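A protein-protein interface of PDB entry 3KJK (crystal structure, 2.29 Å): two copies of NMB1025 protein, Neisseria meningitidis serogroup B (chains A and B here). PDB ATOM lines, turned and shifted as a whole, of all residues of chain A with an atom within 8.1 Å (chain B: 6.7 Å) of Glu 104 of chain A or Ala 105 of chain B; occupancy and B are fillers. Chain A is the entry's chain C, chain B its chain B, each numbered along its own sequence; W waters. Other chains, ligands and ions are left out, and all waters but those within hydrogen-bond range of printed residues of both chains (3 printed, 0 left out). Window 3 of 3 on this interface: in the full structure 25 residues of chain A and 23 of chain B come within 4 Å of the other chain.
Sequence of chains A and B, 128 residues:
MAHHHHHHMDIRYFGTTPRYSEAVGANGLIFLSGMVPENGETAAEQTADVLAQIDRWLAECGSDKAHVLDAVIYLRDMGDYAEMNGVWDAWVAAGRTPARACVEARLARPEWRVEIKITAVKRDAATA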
ATOM      1  N   ILE A  73       1.912 -12.340  12.596  1.00  0.00           N
ATOM      2  CA  ILE A  73       1.965 -13.087  13.839  1.00  0.00           C
ATOM      3  C   ILE A  73       3.232 -12.700  14.593  1.00  0.00           C
ATOM      4  O   ILE A  73       4.347 -12.892  14.100  1.00  0.00           O
ATOM      5  CB  ILE A  73       1.928 -14.618  13.574  1.00  0.00           C
ATOM      6  CG1 ILE A  73       0.686 -14.986  12.747  1.00  0.00           C
ATOM      7  CG2 ILE A  73       1.938 -15.401  14.885  1.00  0.00           C
ATOM      8  CD1 ILE A  73       0.707 -16.383  12.184  1.00  0.00           C
ATOM      9  N   TYR A  74       3.057 -12.137  15.780  1.00  0.00           N
ATOM     10  CA  TYR A  74       4.190 -11.767  16.611  1.00  0.00           C
ATOM     11  C   TYR A  74       4.384 -12.812  17.689  1.00  0.00           C
ATOM     12  O   TYR A  74       3.475 -13.042  18.492  1.00  0.00           O
ATOM     13  CB  TYR A  74       3.970 -10.396  17.255  1.00  0.00           C
ATOM     14  CG  TYR A  74       3.705  -9.293  16.269  1.00  0.00           C
ATOM     15  CD1 TYR A  74       4.755  -8.670  15.589  1.00  0.00           C
ATOM     16  CD2 TYR A  74       2.398  -8.869  16.008  1.00  0.00           C
ATOM     17  CE1 TYR A  74       4.515  -7.649  14.683  1.00  0.00           C
ATOM     18  CE2 TYR A  74       2.147  -7.849  15.102  1.00  0.00           C
ATOM     19  CZ  TYR A  74       3.208  -7.241  14.445  1.00  0.00           C
ATOM     20  OH  TYR A  74       2.953  -6.233  13.545  1.00  0.00           O
ATOM     21  N   LEU A  75       5.554 -13.451  17.696  1.00  0.00           N
ATOM     22  CA  LEU A  75       5.922 -14.365  18.774  1.00  0.00           C
ATOM     23  C   LEU A  75       6.912 -13.698  19.718  1.00  0.00           C
ATOM     24  O   LEU A  75       7.860 -13.055  19.271  1.00  0.00           O
ATOM     25  CB  LEU A  75       6.539 -15.650  18.223  1.00  0.00           C
ATOM     26  CG  LEU A  75       5.611 -16.579  17.447  1.00  0.00           C
ATOM     27  CD1 LEU A  75       6.408 -17.682  16.762  1.00  0.00           C
ATOM     28  CD2 LEU A  75       4.532 -17.162  18.368  1.00  0.00           C
ATOM     29  N   ARG A  76       6.699 -13.854  21.019  1.00  0.00           N
ATOM     30  CA  ARG A  76       7.678 -13.387  21.982  1.00  0.00           C
ATOM     31  C   ARG A  76       9.003 -14.119  21.755  1.00  0.00           C
ATOM     32  O   ARG A  76      10.070 -13.496  21.744  1.00  0.00           O
ATOM     33  CB  ARG A  76       7.180 -13.591  23.406  1.00  0.00           C
ATOM     34  CG  ARG A  76       8.202 -13.231  24.470  1.00  0.00           C
ATOM     35  CD  ARG A  76       7.695 -13.595  25.861  1.00  0.00           C
ATOM     36  NE  ARG A  76       8.681 -13.324  26.905  1.00  0.00           N
ATOM     37  CZ  ARG A  76       8.947 -12.120  27.410  1.00  0.00           C
ATOM     38  NH1 ARG A  76       8.311 -11.037  26.976  1.00  0.00           N
ATOM     39  NH2 ARG A  76       9.857 -12.002  28.366  1.00  0.00           N
ATOM     40  N   ASP A  77       8.914 -15.431  21.535  1.00  0.00           N
ATOM     41  CA  ASP A  77      10.083 -16.296  21.361  1.00  0.00           C
ATOM     42  C   ASP A  77       9.887 -17.181  20.134  1.00  0.00           C
ATOM     43  O   ASP A  77       8.954 -17.995  20.094  1.00  0.00           O
ATOM     44  CB  ASP A  77      10.270 -17.171  22.612  1.00  0.00           C
ATOM     45  CG  ASP A  77      11.641 -17.837  22.680  1.00  0.00           C
ATOM     46  OD1 ASP A  77      12.136 -18.038  23.812  1.00  0.00           O
ATOM     47  OD2 ASP A  77      12.223 -18.169  21.625  1.00  0.00           O
ATOM     48  N   MET A  78      10.772 -17.035  19.149  1.00  0.00           N
ATOM     49  CA  MET A  78      10.689 -17.791  17.893  1.00  0.00           C
ATOM     50  C   MET A  78      10.856 -19.303  18.107  1.00  0.00           C
ATOM     51  O   MET A  78      10.573 -20.107  17.212  1.00  0.00           O
ATOM     52  CB  MET A  78      11.715 -17.275  16.878  1.00  0.00           C
ATOM     53  CG  MET A  78      11.546 -17.825  15.473  1.00  0.00           C
ATOM     54  SD  MET A  78       9.783 -17.419  14.717  1.00  0.00           S
ATOM     55  CE  MET A  78       9.941 -15.482  14.611  1.00  0.00           C
ATOM     56  N   GLY A  79      11.302 -19.684  19.299  1.00  0.00           N
ATOM     57  CA  GLY A  79      11.362 -21.093  19.685  1.00  0.00           C
ATOM     58  C   GLY A  79       9.982 -21.724  19.726  1.00  0.00           C
ATOM     59  O   GLY A  79       9.863 -22.943  19.711  1.00  0.00           O
ATOM     60  N   ASP A  80       8.947 -20.882  19.766  1.00  0.00           N
ATOM     61  CA  ASP A  80       7.552 -21.321  19.829  1.00  0.00           C
ATOM     62  C   ASP A  80       6.925 -21.469  18.441  1.00  0.00           C
ATOM     63  O   ASP A  80       5.717 -21.693  18.314  1.00  0.00           O
ATOM     64  CB  ASP A  80       6.726 -20.331  20.666  1.00  0.00           C
ATOM     65  CG  ASP A  80       6.880 -20.549  22.174  1.00  0.00           C
ATOM     66  OD1 ASP A  80       7.367 -21.623  22.589  1.00  0.00           O
ATOM     67  OD2 ASP A  80       6.504 -19.640  22.950  1.00  0.00           O
ATOM     68  N   ALA A 101       2.843 -13.272   7.717  1.00  0.00           N
ATOM     69  CA  ALA A 101       4.201 -12.983   8.148  1.00  0.00           C
ATOM     70  C   ALA A 101       4.286 -13.320   9.619  1.00  0.00           C
ATOM     71  O   ALA A 101       3.327 -13.092  10.363  1.00  0.00           O
ATOM     72  CB  ALA A 101       4.536 -11.525   7.931  1.00  0.00           C
ATOM     73  N   CYS A 102       5.423 -13.870  10.038  1.00  0.00           N
ATOM     74  CA  CYS A 102       5.654 -14.177  11.444  1.00  0.00           C
ATOM     75  C   CYS A 102       7.031 -13.694  11.873  1.00  0.00           C
ATOM     76  O   CYS A 102       8.038 -14.077  11.287  1.00  0.00           O
ATOM     77  CB  CYS A 102       5.501 -15.676  11.704  1.00  0.00           C
ATOM     78  SG  CYS A 102       5.992 -16.180  13.384  1.00  0.00           S
ATOM     79  N   VAL A 103       7.066 -12.842  12.894  1.00  0.00           N
ATOM     80  CA  VAL A 103       8.318 -12.272  13.393  1.00  0.00           C
ATOM     81  C   VAL A 103       8.345 -12.289  14.917  1.00  0.00           C
ATOM     82  O   VAL A 103       7.308 -12.445  15.572  1.00  0.00           O
ATOM     83  CB  VAL A 103       8.569 -10.822  12.877  1.00  0.00           C
ATOM     84  CG1 VAL A 103       8.625 -10.771  11.336  1.00  0.00           C
ATOM     85  CG2 VAL A 103       7.522  -9.845  13.416  1.00  0.00           C
ATOM     86  N   GLU A 104       9.540 -12.132  15.477  1.00  0.00           N
ATOM     87  CA  GLU A 104       9.724 -12.216  16.910  1.00  0.00           C
ATOM     88  C   GLU A 104       9.745 -10.829  17.534  1.00  0.00           C
ATOM     89  O   GLU A 104      10.598  -9.998  17.212  1.00  0.00           O
ATOM     90  CB  GLU A 104      11.011 -12.968  17.235  1.00  0.00           C
ATOM     91  CG  GLU A 104      11.056 -13.527  18.647  1.00  0.00           C
ATOM     92  CD  GLU A 104      12.464 -13.889  19.083  1.00  0.00           C
ATOM     93  OE1 GLU A 104      13.303 -12.977  19.236  1.00  0.00           O
ATOM     94  OE2 GLU A 104      12.729 -15.089  19.280  1.00  0.00           O
ATOM     95  N   ALA A 105       8.789 -10.584  18.421  1.00  0.00           N
ATOM     96  CA  ALA A 105       8.709  -9.319  19.131  1.00  0.00           C
ATOM     97  C   ALA A 105       8.097  -9.559  20.505  1.00  0.00           C
ATOM     98  O   ALA A 105       7.095 -10.272  20.626  1.00  0.00           O
ATOM     99  CB  ALA A 105       7.873  -8.304  18.318  1.00  0.00           C
ATOM    100  N   ARG A 106       8.710  -8.997  21.545  1.00  0.00           N
ATOM    101  CA  ARG A 106       8.134  -9.060  22.892  1.00  0.00           C
ATOM    102  C   ARG A 106       6.807  -8.302  22.912  1.00  0.00           C
ATOM    103  O   ARG A 106       6.638  -7.337  22.183  1.00  0.00           O
ATOM    104  CB  ARG A 106       9.112  -8.524  23.956  1.00  0.00           C
ATOM    105  CG  ARG A 106      10.355  -9.405  24.154  1.00  0.00           C
ATOM    106  CD  ARG A 106      11.084  -9.176  25.480  1.00  0.00           C
ATOM    107  NE  ARG A 106      12.342  -9.926  25.516  1.00  0.00           N
ATOM    108  CZ  ARG A 106      12.702 -10.803  26.456  1.00  0.00           C
ATOM    109  NH1 ARG A 106      13.860 -11.436  26.364  1.00  0.00           N
ATOM    110  NH2 ARG A 106      11.923 -11.049  27.493  1.00  0.00           N
ATOM    111  N   LEU A 107       5.864  -8.758  23.727  1.00  0.00           N
ATOM    112  CA  LEU A 107       4.536  -8.138  23.789  1.00  0.00           C
ATOM    113  C   LEU A 107       4.324  -7.327  25.087  1.00  0.00           C
ATOM    114  O   LEU A 107       5.256  -7.187  25.887  1.00  0.00           O
ATOM    115  CB  LEU A 107       3.454  -9.197  23.562  1.00  0.00           C
ATOM    116  CG  LEU A 107       3.762 -10.107  22.366  1.00  0.00           C
ATOM    117  CD1 LEU A 107       2.862 -11.328  22.316  1.00  0.00           C
ATOM    118  CD2 LEU A 107       3.698  -9.348  21.041  1.00  0.00           C
ATOM    119  N   ARG A 113       2.743 -15.027  24.804  1.00  0.00           N
ATOM    120  CA  ARG A 113       3.670 -15.683  23.868  1.00  0.00           C
ATOM    121  C   ARG A 113       3.381 -15.345  22.419  1.00  0.00           C
ATOM    122  O   ARG A 113       4.240 -15.468  21.569  1.00  0.00           O
ATOM    123  CB  ARG A 113       3.665 -17.214  24.021  1.00  0.00           C
ATOM    124  CG  ARG A 113       3.715 -17.763  25.440  1.00  0.00           C
ATOM    125  CD  ARG A 113       5.044 -17.552  26.152  1.00  0.00           C
ATOM    126  NE  ARG A 113       6.193 -18.146  25.470  1.00  0.00           N
ATOM    127  CZ  ARG A 113       7.406 -18.273  26.008  1.00  0.00           C
ATOM    128  NH1 ARG A 113       8.386 -18.820  25.304  1.00  0.00           N
ATOM    129  NH2 ARG A 113       7.644 -17.870  27.251  1.00  0.00           N
ATOM    130  N   ILE B  73       9.693  -3.602   6.508  1.00  0.00           N
ATOM    131  CA  ILE B  73      10.945  -4.329   6.401  1.00  0.00           C
ATOM    132  C   ILE B  73      11.397  -4.752   7.781  1.00  0.00           C
ATOM    133  O   ILE B  73      11.636  -3.910   8.653  1.00  0.00           O
ATOM    134  CB  ILE B  73      12.028  -3.478   5.708  1.00  0.00           C
ATOM    135  CG1 ILE B  73      11.544  -3.060   4.314  1.00  0.00           C
ATOM    136  CG2 ILE B  73      13.329  -4.248   5.598  1.00  0.00           C
ATOM    137  CD1 ILE B  73      12.346  -1.939   3.691  1.00  0.00           C
ATOM    138  N   TYR B  74      11.495  -6.063   7.987  1.00  0.00           N
ATOM    139  CA  TYR B  74      12.013  -6.585   9.248  1.00  0.00           C
ATOM    140  C   TYR B  74      13.446  -7.064   9.070  1.00  0.00           C
ATOM    141  O   TYR B  74      13.727  -7.884   8.198  1.00  0.00           O
ATOM    142  CB  TYR B  74      11.160  -7.732   9.779  1.00  0.00           C
ATOM    143  CG  TYR B  74       9.681  -7.459   9.872  1.00  0.00           C
ATOM    144  CD1 TYR B  74       9.133  -6.837  10.993  1.00  0.00           C
ATOM    145  CD2 TYR B  74       8.818  -7.867   8.858  1.00  0.00           C
ATOM    146  CE1 TYR B  74       7.756  -6.604  11.089  1.00  0.00           C
ATOM    147  CE2 TYR B  74       7.451  -7.640   8.942  1.00  0.00           C
ATOM    148  CZ  TYR B  74       6.927  -7.015  10.058  1.00  0.00           C
ATOM    149  OH  TYR B  74       5.575  -6.801  10.128  1.00  0.00           O
ATOM    150  N   LEU B  75      14.341  -6.544   9.901  1.00  0.00           N
ATOM    151  CA  LEU B  75      15.739  -6.942   9.883  1.00  0.00           C
ATOM    152  C   LEU B  75      16.036  -7.690  11.164  1.00  0.00           C
ATOM    153  O   LEU B  75      15.662  -7.225  12.236  1.00  0.00           O
ATOM    154  CB  LEU B  75      16.658  -5.712   9.774  1.00  0.00           C
ATOM    155  CG  LEU B  75      16.690  -4.938   8.443  1.00  0.00           C
ATOM    156  CD1 LEU B  75      17.521  -3.657   8.546  1.00  0.00           C
ATOM    157  CD2 LEU B  75      17.216  -5.815   7.318  1.00  0.00           C
ATOM    158  N   ARG B  76      16.703  -8.841  11.052  1.00  0.00           N
ATOM    159  CA  ARG B  76      17.195  -9.564  12.231  1.00  0.00           C
ATOM    160  C   ARG B  76      18.083  -8.651  13.082  1.00  0.00           C
ATOM    161  O   ARG B  76      18.007  -8.669  14.319  1.00  0.00           O
ATOM    162  CB  ARG B  76      17.938 -10.865  11.845  1.00  0.00           C
ATOM    163  CG  ARG B  76      19.034 -11.300  12.837  1.00  0.00           C
ATOM    164  CD  ARG B  76      19.567 -12.727  12.618  1.00  0.00           C
ATOM    165  NE  ARG B  76      18.644 -13.694  13.195  1.00  0.00           N
ATOM    166  CZ  ARG B  76      18.869 -14.463  14.258  1.00  0.00           C
ATOM    167  NH1 ARG B  76      17.912 -15.272  14.670  1.00  0.00           N
ATOM    168  NH2 ARG B  76      20.026 -14.456  14.903  1.00  0.00           N
ATOM    169  N   ASP B  77      18.891  -7.836  12.407  1.00  0.00           N
ATOM    170  CA  ASP B  77      19.918  -7.021  13.060  1.00  0.00           C
ATOM    171  C   ASP B  77      19.986  -5.646  12.404  1.00  0.00           C
ATOM    172  O   ASP B  77      20.359  -5.537  11.229  1.00  0.00           O
ATOM    173  CB  ASP B  77      21.280  -7.727  12.956  1.00  0.00           C
ATOM    174  CG  ASP B  77      22.353  -7.089  13.824  1.00  0.00           C
ATOM    175  OD1 ASP B  77      23.132  -7.849  14.435  1.00  0.00           O
ATOM    176  OD2 ASP B  77      22.441  -5.842  13.890  1.00  0.00           O
ATOM    177  N   MET B  78      19.630  -4.610  13.169  1.00  0.00           N
ATOM    178  CA  MET B  78      19.574  -3.226  12.680  1.00  0.00           C
ATOM    179  C   MET B  78      20.946  -2.707  12.221  1.00  0.00           C
ATOM    180  O   MET B  78      21.038  -1.655  11.597  1.00  0.00           O
ATOM    181  CB  MET B  78      18.938  -2.296  13.737  1.00  0.00           C
ATOM    182  CG  MET B  78      18.552  -0.898  13.231  1.00  0.00           C
ATOM    183  SD  MET B  78      17.335  -0.846  11.682  1.00  0.00           S
ATOM    184  CE  MET B  78      15.711  -1.450  12.568  1.00  0.00           C
ATOM    185  N   VAL B 103      11.874  -2.058  10.990  1.00  0.00           N
ATOM    186  CA  VAL B 103      12.093  -2.361  12.410  1.00  0.00           C
ATOM    187  C   VAL B 103      12.881  -3.663  12.555  1.00  0.00           C
ATOM    188  O   VAL B 103      12.969  -4.467  11.615  1.00  0.00           O
ATOM    189  CB  VAL B 103      10.777  -2.456  13.242  1.00  0.00           C
ATOM    190  CG1 VAL B 103       9.858  -1.278  12.959  1.00  0.00           C
ATOM    191  CG2 VAL B 103      10.047  -3.774  12.986  1.00  0.00           C
ATOM    192  N   GLU B 104      13.449  -3.856  13.740  1.00  0.00           N
ATOM    193  CA  GLU B 104      14.274  -5.015  14.024  1.00  0.00           C
ATOM    194  C   GLU B 104      13.482  -6.114  14.727  1.00  0.00           C
ATOM    195  O   GLU B 104      12.997  -5.931  15.844  1.00  0.00           O
ATOM    196  CB  GLU B 104      15.474  -4.603  14.870  1.00  0.00           C
ATOM    197  CG  GLU B 104      16.577  -5.640  14.915  1.00  0.00           C
ATOM    198  CD  GLU B 104      17.589  -5.349  15.999  1.00  0.00           C
ATOM    199  OE1 GLU B 104      17.242  -5.506  17.187  1.00  0.00           O
ATOM    200  OE2 GLU B 104      18.728  -4.964  15.664  1.00  0.00           O
ATOM    201  N   ALA B 105      13.353  -7.249  14.046  1.00  0.00           N
ATOM    202  CA  ALA B 105      12.721  -8.441  14.601  1.00  0.00           C
ATOM    203  C   ALA B 105      13.367  -9.702  14.016  1.00  0.00           C
ATOM    204  O   ALA B 105      13.586  -9.796  12.799  1.00  0.00           O
ATOM    205  CB  ALA B 105      11.230  -8.427  14.326  1.00  0.00           C
ATOM    206  N   ARG B 106      13.676 -10.665  14.880  1.00  0.00           N
ATOM    207  CA  ARG B 106      14.242 -11.936  14.446  1.00  0.00           C
ATOM    208  C   ARG B 106      13.216 -12.690  13.631  1.00  0.00           C
ATOM    209  O   ARG B 106      12.026 -12.572  13.864  1.00  0.00           O
ATOM    210  CB  ARG B 106      14.682 -12.781  15.638  1.00  0.00           C
ATOM    211  CG  ARG B 106      15.706 -12.104  16.523  1.00  0.00           C
ATOM    212  CD  ARG B 106      16.627 -13.109  17.157  1.00  0.00           C
ATOM    213  NE  ARG B 106      17.025 -12.671  18.484  1.00  0.00           N
ATOM    214  CZ  ARG B 106      18.221 -12.877  19.022  1.00  0.00           C
ATOM    215  NH1 ARG B 106      18.467 -12.414  20.247  1.00  0.00           N
ATOM    216  NH2 ARG B 106      19.170 -13.525  18.341  1.00  0.00           N
ATOM    217  N   LEU B 107      13.689 -13.465  12.672  1.00  0.00           N
ATOM    218  CA  LEU B 107      12.798 -14.148  11.748  1.00  0.00           C
ATOM    219  C   LEU B 107      12.762 -15.657  12.021  1.00  0.00           C
ATOM    220  O   LEU B 107      13.450 -16.146  12.928  1.00  0.00           O
ATOM    221  CB  LEU B 107      13.201 -13.806  10.303  1.00  0.00           C
ATOM    222  CG  LEU B 107      13.510 -12.313  10.104  1.00  0.00           C
ATOM    223  CD1 LEU B 107      14.257 -12.063   8.801  1.00  0.00           C
ATOM    224  CD2 LEU B 107      12.248 -11.453  10.176  1.00  0.00           C
ATOM    225  N   ALA B 108      11.957 -16.382  11.243  1.00  0.00           N
ATOM    226  CA  ALA B 108      11.690 -17.816  11.466  1.00  0.00           C
ATOM    227  C   ALA B 108      12.919 -18.732  11.367  1.00  0.00           C
ATOM    228  O   ALA B 108      12.936 -19.815  11.952  1.00  0.00           O
ATOM    229  CB  ALA B 108      10.577 -18.307  10.532  1.00  0.00           C
ATOM    230  N   TRP B 112      18.125 -15.940   8.267  1.00  0.00           N
ATOM    231  CA  TRP B 112      17.383 -14.896   7.562  1.00  0.00           C
ATOM    232  C   TRP B 112      17.652 -13.535   8.192  1.00  0.00           C
ATOM    233  O   TRP B 112      17.341 -13.305   9.360  1.00  0.00           O
ATOM    234  CB  TRP B 112      15.877 -15.187   7.518  1.00  0.00           C
ATOM    235  CG  TRP B 112      15.494 -16.441   6.790  1.00  0.00           C
ATOM    236  CD1 TRP B 112      16.268 -17.166   5.925  1.00  0.00           C
ATOM    237  CD2 TRP B 112      14.218 -17.091   6.825  1.00  0.00           C
ATOM    238  NE1 TRP B 112      15.556 -18.238   5.434  1.00  0.00           N
ATOM    239  CE2 TRP B 112      14.294 -18.213   5.968  1.00  0.00           C
ATOM    240  CE3 TRP B 112      13.013 -16.831   7.496  1.00  0.00           C
ATOM    241  CZ2 TRP B 112      13.211 -19.081   5.768  1.00  0.00           C
ATOM    242  CZ3 TRP B 112      11.938 -17.690   7.298  1.00  0.00           C
ATOM    243  CH2 TRP B 112      12.047 -18.808   6.446  1.00  0.00           C
ATOM    244  N   ARG B 113      18.241 -12.645   7.405  1.00  0.00           N
ATOM    245  CA  ARG B 113      18.654 -11.342   7.898  1.00  0.00           C
ATOM    246  C   ARG B 113      17.632 -10.251   7.575  1.00  0.00           C
ATOM    247  O   ARG B 113      17.677  -9.170   8.166  1.00  0.00           O
ATOM    248  CB  ARG B 113      20.039 -10.985   7.353  1.00  0.00           C
ATOM    249  CG  ARG B 113      21.086 -12.075   7.621  1.00  0.00           C
ATOM    250  CD  ARG B 113      22.522 -11.545   7.578  1.00  0.00           C
ATOM    251  NE  ARG B 113      22.777 -10.533   8.607  1.00  0.00           N
ATOM    252  CZ  ARG B 113      23.085 -10.794   9.877  1.00  0.00           C
ATOM    253  NH1 ARG B 113      23.291  -9.793  10.723  1.00  0.00           N
ATOM    254  NH2 ARG B 113      23.184 -12.047  10.308  1.00  0.00           N
HETATM  255  O   HOH W   1      13.278  -9.848  18.143  1.00  0.00           O
HETATM  256  O   HOH W   2      11.832  -7.407  17.972  1.00  0.00           O
HETATM  257  O   HOH W   3       4.619  -5.183  11.883  1.00  0.00           O
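Of the 16 printed residues of chain A, 3 touch a printed residue of chain B.
Along chain A the printed residues that touch a printed residue of chain B span positions 78 to 104.
Of the 14 printed residues of chain B, 5 touch a printed residue of chain A.
Printed residues of chain B that touch a printed residue of chain A: Tyr 74, Ala 105, Arg 106, Leu 107 and Ala 108.
Among the printed residues, Asp or Glu carboxylates within 4 Å of a Lys or Arg side-chain nitrogen of the other chain: Glu 104 of chain A with Arg 106 of chain B (3.8 Å).
Val 103 of chain A touches Ala 105 of chain B, but with the chains exchanged Ala 105 of chain A does not touch Val 103 of chain B (7.3 Å).
Val 103 of chain A touches Arg 106 of chain B, but with the chains exchanged Arg 106 of chain A does not touch Val 103 of chain B (10.1 Å).
Glu 104 of chain A touches Ala 105 of chain B, but with the chains exchanged Ala 105 of chain A does not touch Glu 104 of chain B (6.2 Å).
Glu 104 of chain A touches Arg 106 of chain B, but with the chains exchanged Arg 106 of chain A does not touch Glu 104 of chain B (7.8 Å).
Of the 9 pairs that touch across the chains among the printed residues, none has its exchanged pair printed and touching as well.
Of chain A, only Val 103 and Glu 104 come within 4 Å of Ala 105 of chain B.
Printed residues of chain A within 4 Å of Leu 107 of chain B: Met 78 and Val 103.
Printed residues of chain B within 4 Å of Val 103 of chain A: Tyr 74, Ala 105, Arg 106 and Leu 107.
Printed residues of chain A within 4 Å of Arg 106 of chain B: Met 78 (3.7 Å), Val 103 (3.7 Å) and Glu 104 (3.0 Å).
Printed residues of chain B within 4 Å of Met 78 of chain A: Arg 106, Leu 107 and Ala 108.
Tyr 74 of chain A touches none of the printed residues of chain B.
The nearest residue of chain B that does not touch Glu 104 of chain A is Glu 104 of chain B (4.9 Å).
The nearest printed residue of chain B that does not touch Met 78 of chain A is Ala 105 of chain B (6.7 Å).
Among the printed residues, pairs that only touch across the chains: Glu 104 of chain A with Ala 105 of chain B (3.3 Å), Met 78 of chain A with Leu 107 of chain B (3.6 Å), Met 78 of chain A with Arg 106 of chain B (3.7 Å), Val 103 of chain A with Arg 106 of chain B (3.7 Å), Val 103 of chain A with Tyr 74 of chain B (3.8 Å), Met 78 of chain A with Ala 108 of chain B (3.8 Å), Val 103 of chain A with Ala 105 of chain B (3.9 Å) and Val 103 of chain A with Leu 107 of chain B (3.9 Å).
The backbone NH (N) of Met 78 of chain A sits at hydrogen-bond distance from the side-chain carboxylate (OE2) of Glu 104 of chain A (2.8 Å).
The backbone carbonyl oxygen of Leu 75 of chain B sits at hydrogen-bond distance from the backbone NH of Ala 105 of chain B.
The backbone carbonyl oxygen of Ile 73 of chain A is in hydrogen-bond range of the backbone NH of Val 103 of chain A, at 3.0 Å.
O of Val 103 of chain A lies within hydrogen-bond range of N of Leu 75 of chain A (2.9 Å).
Water W3 lies within hydrogen-bond range of the side-chain hydroxyl of Tyr 74 of chain B (2.6 Å) and the side-chain hydroxyl of Tyr 74 of chain A (2.6 Å).
Water W2 lies within hydrogen-bond range of the backbone carbonyl oxygen (O) of Glu 104 of chain B (2.8 Å) and the backbone carbonyl oxygen (O) of Glu 104 of chain A (3.0 Å).
Water W1 lies within hydrogen-bond range of O of Glu 104 of chain A (2.8 Å) and N of Arg 106 of chain B (3.4 Å).
The side-chain carboxylate (OE1) of Glu 104 of chain A lies within salt-bridge range of the guanidinium group (NE) of Arg 106 of chain B.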
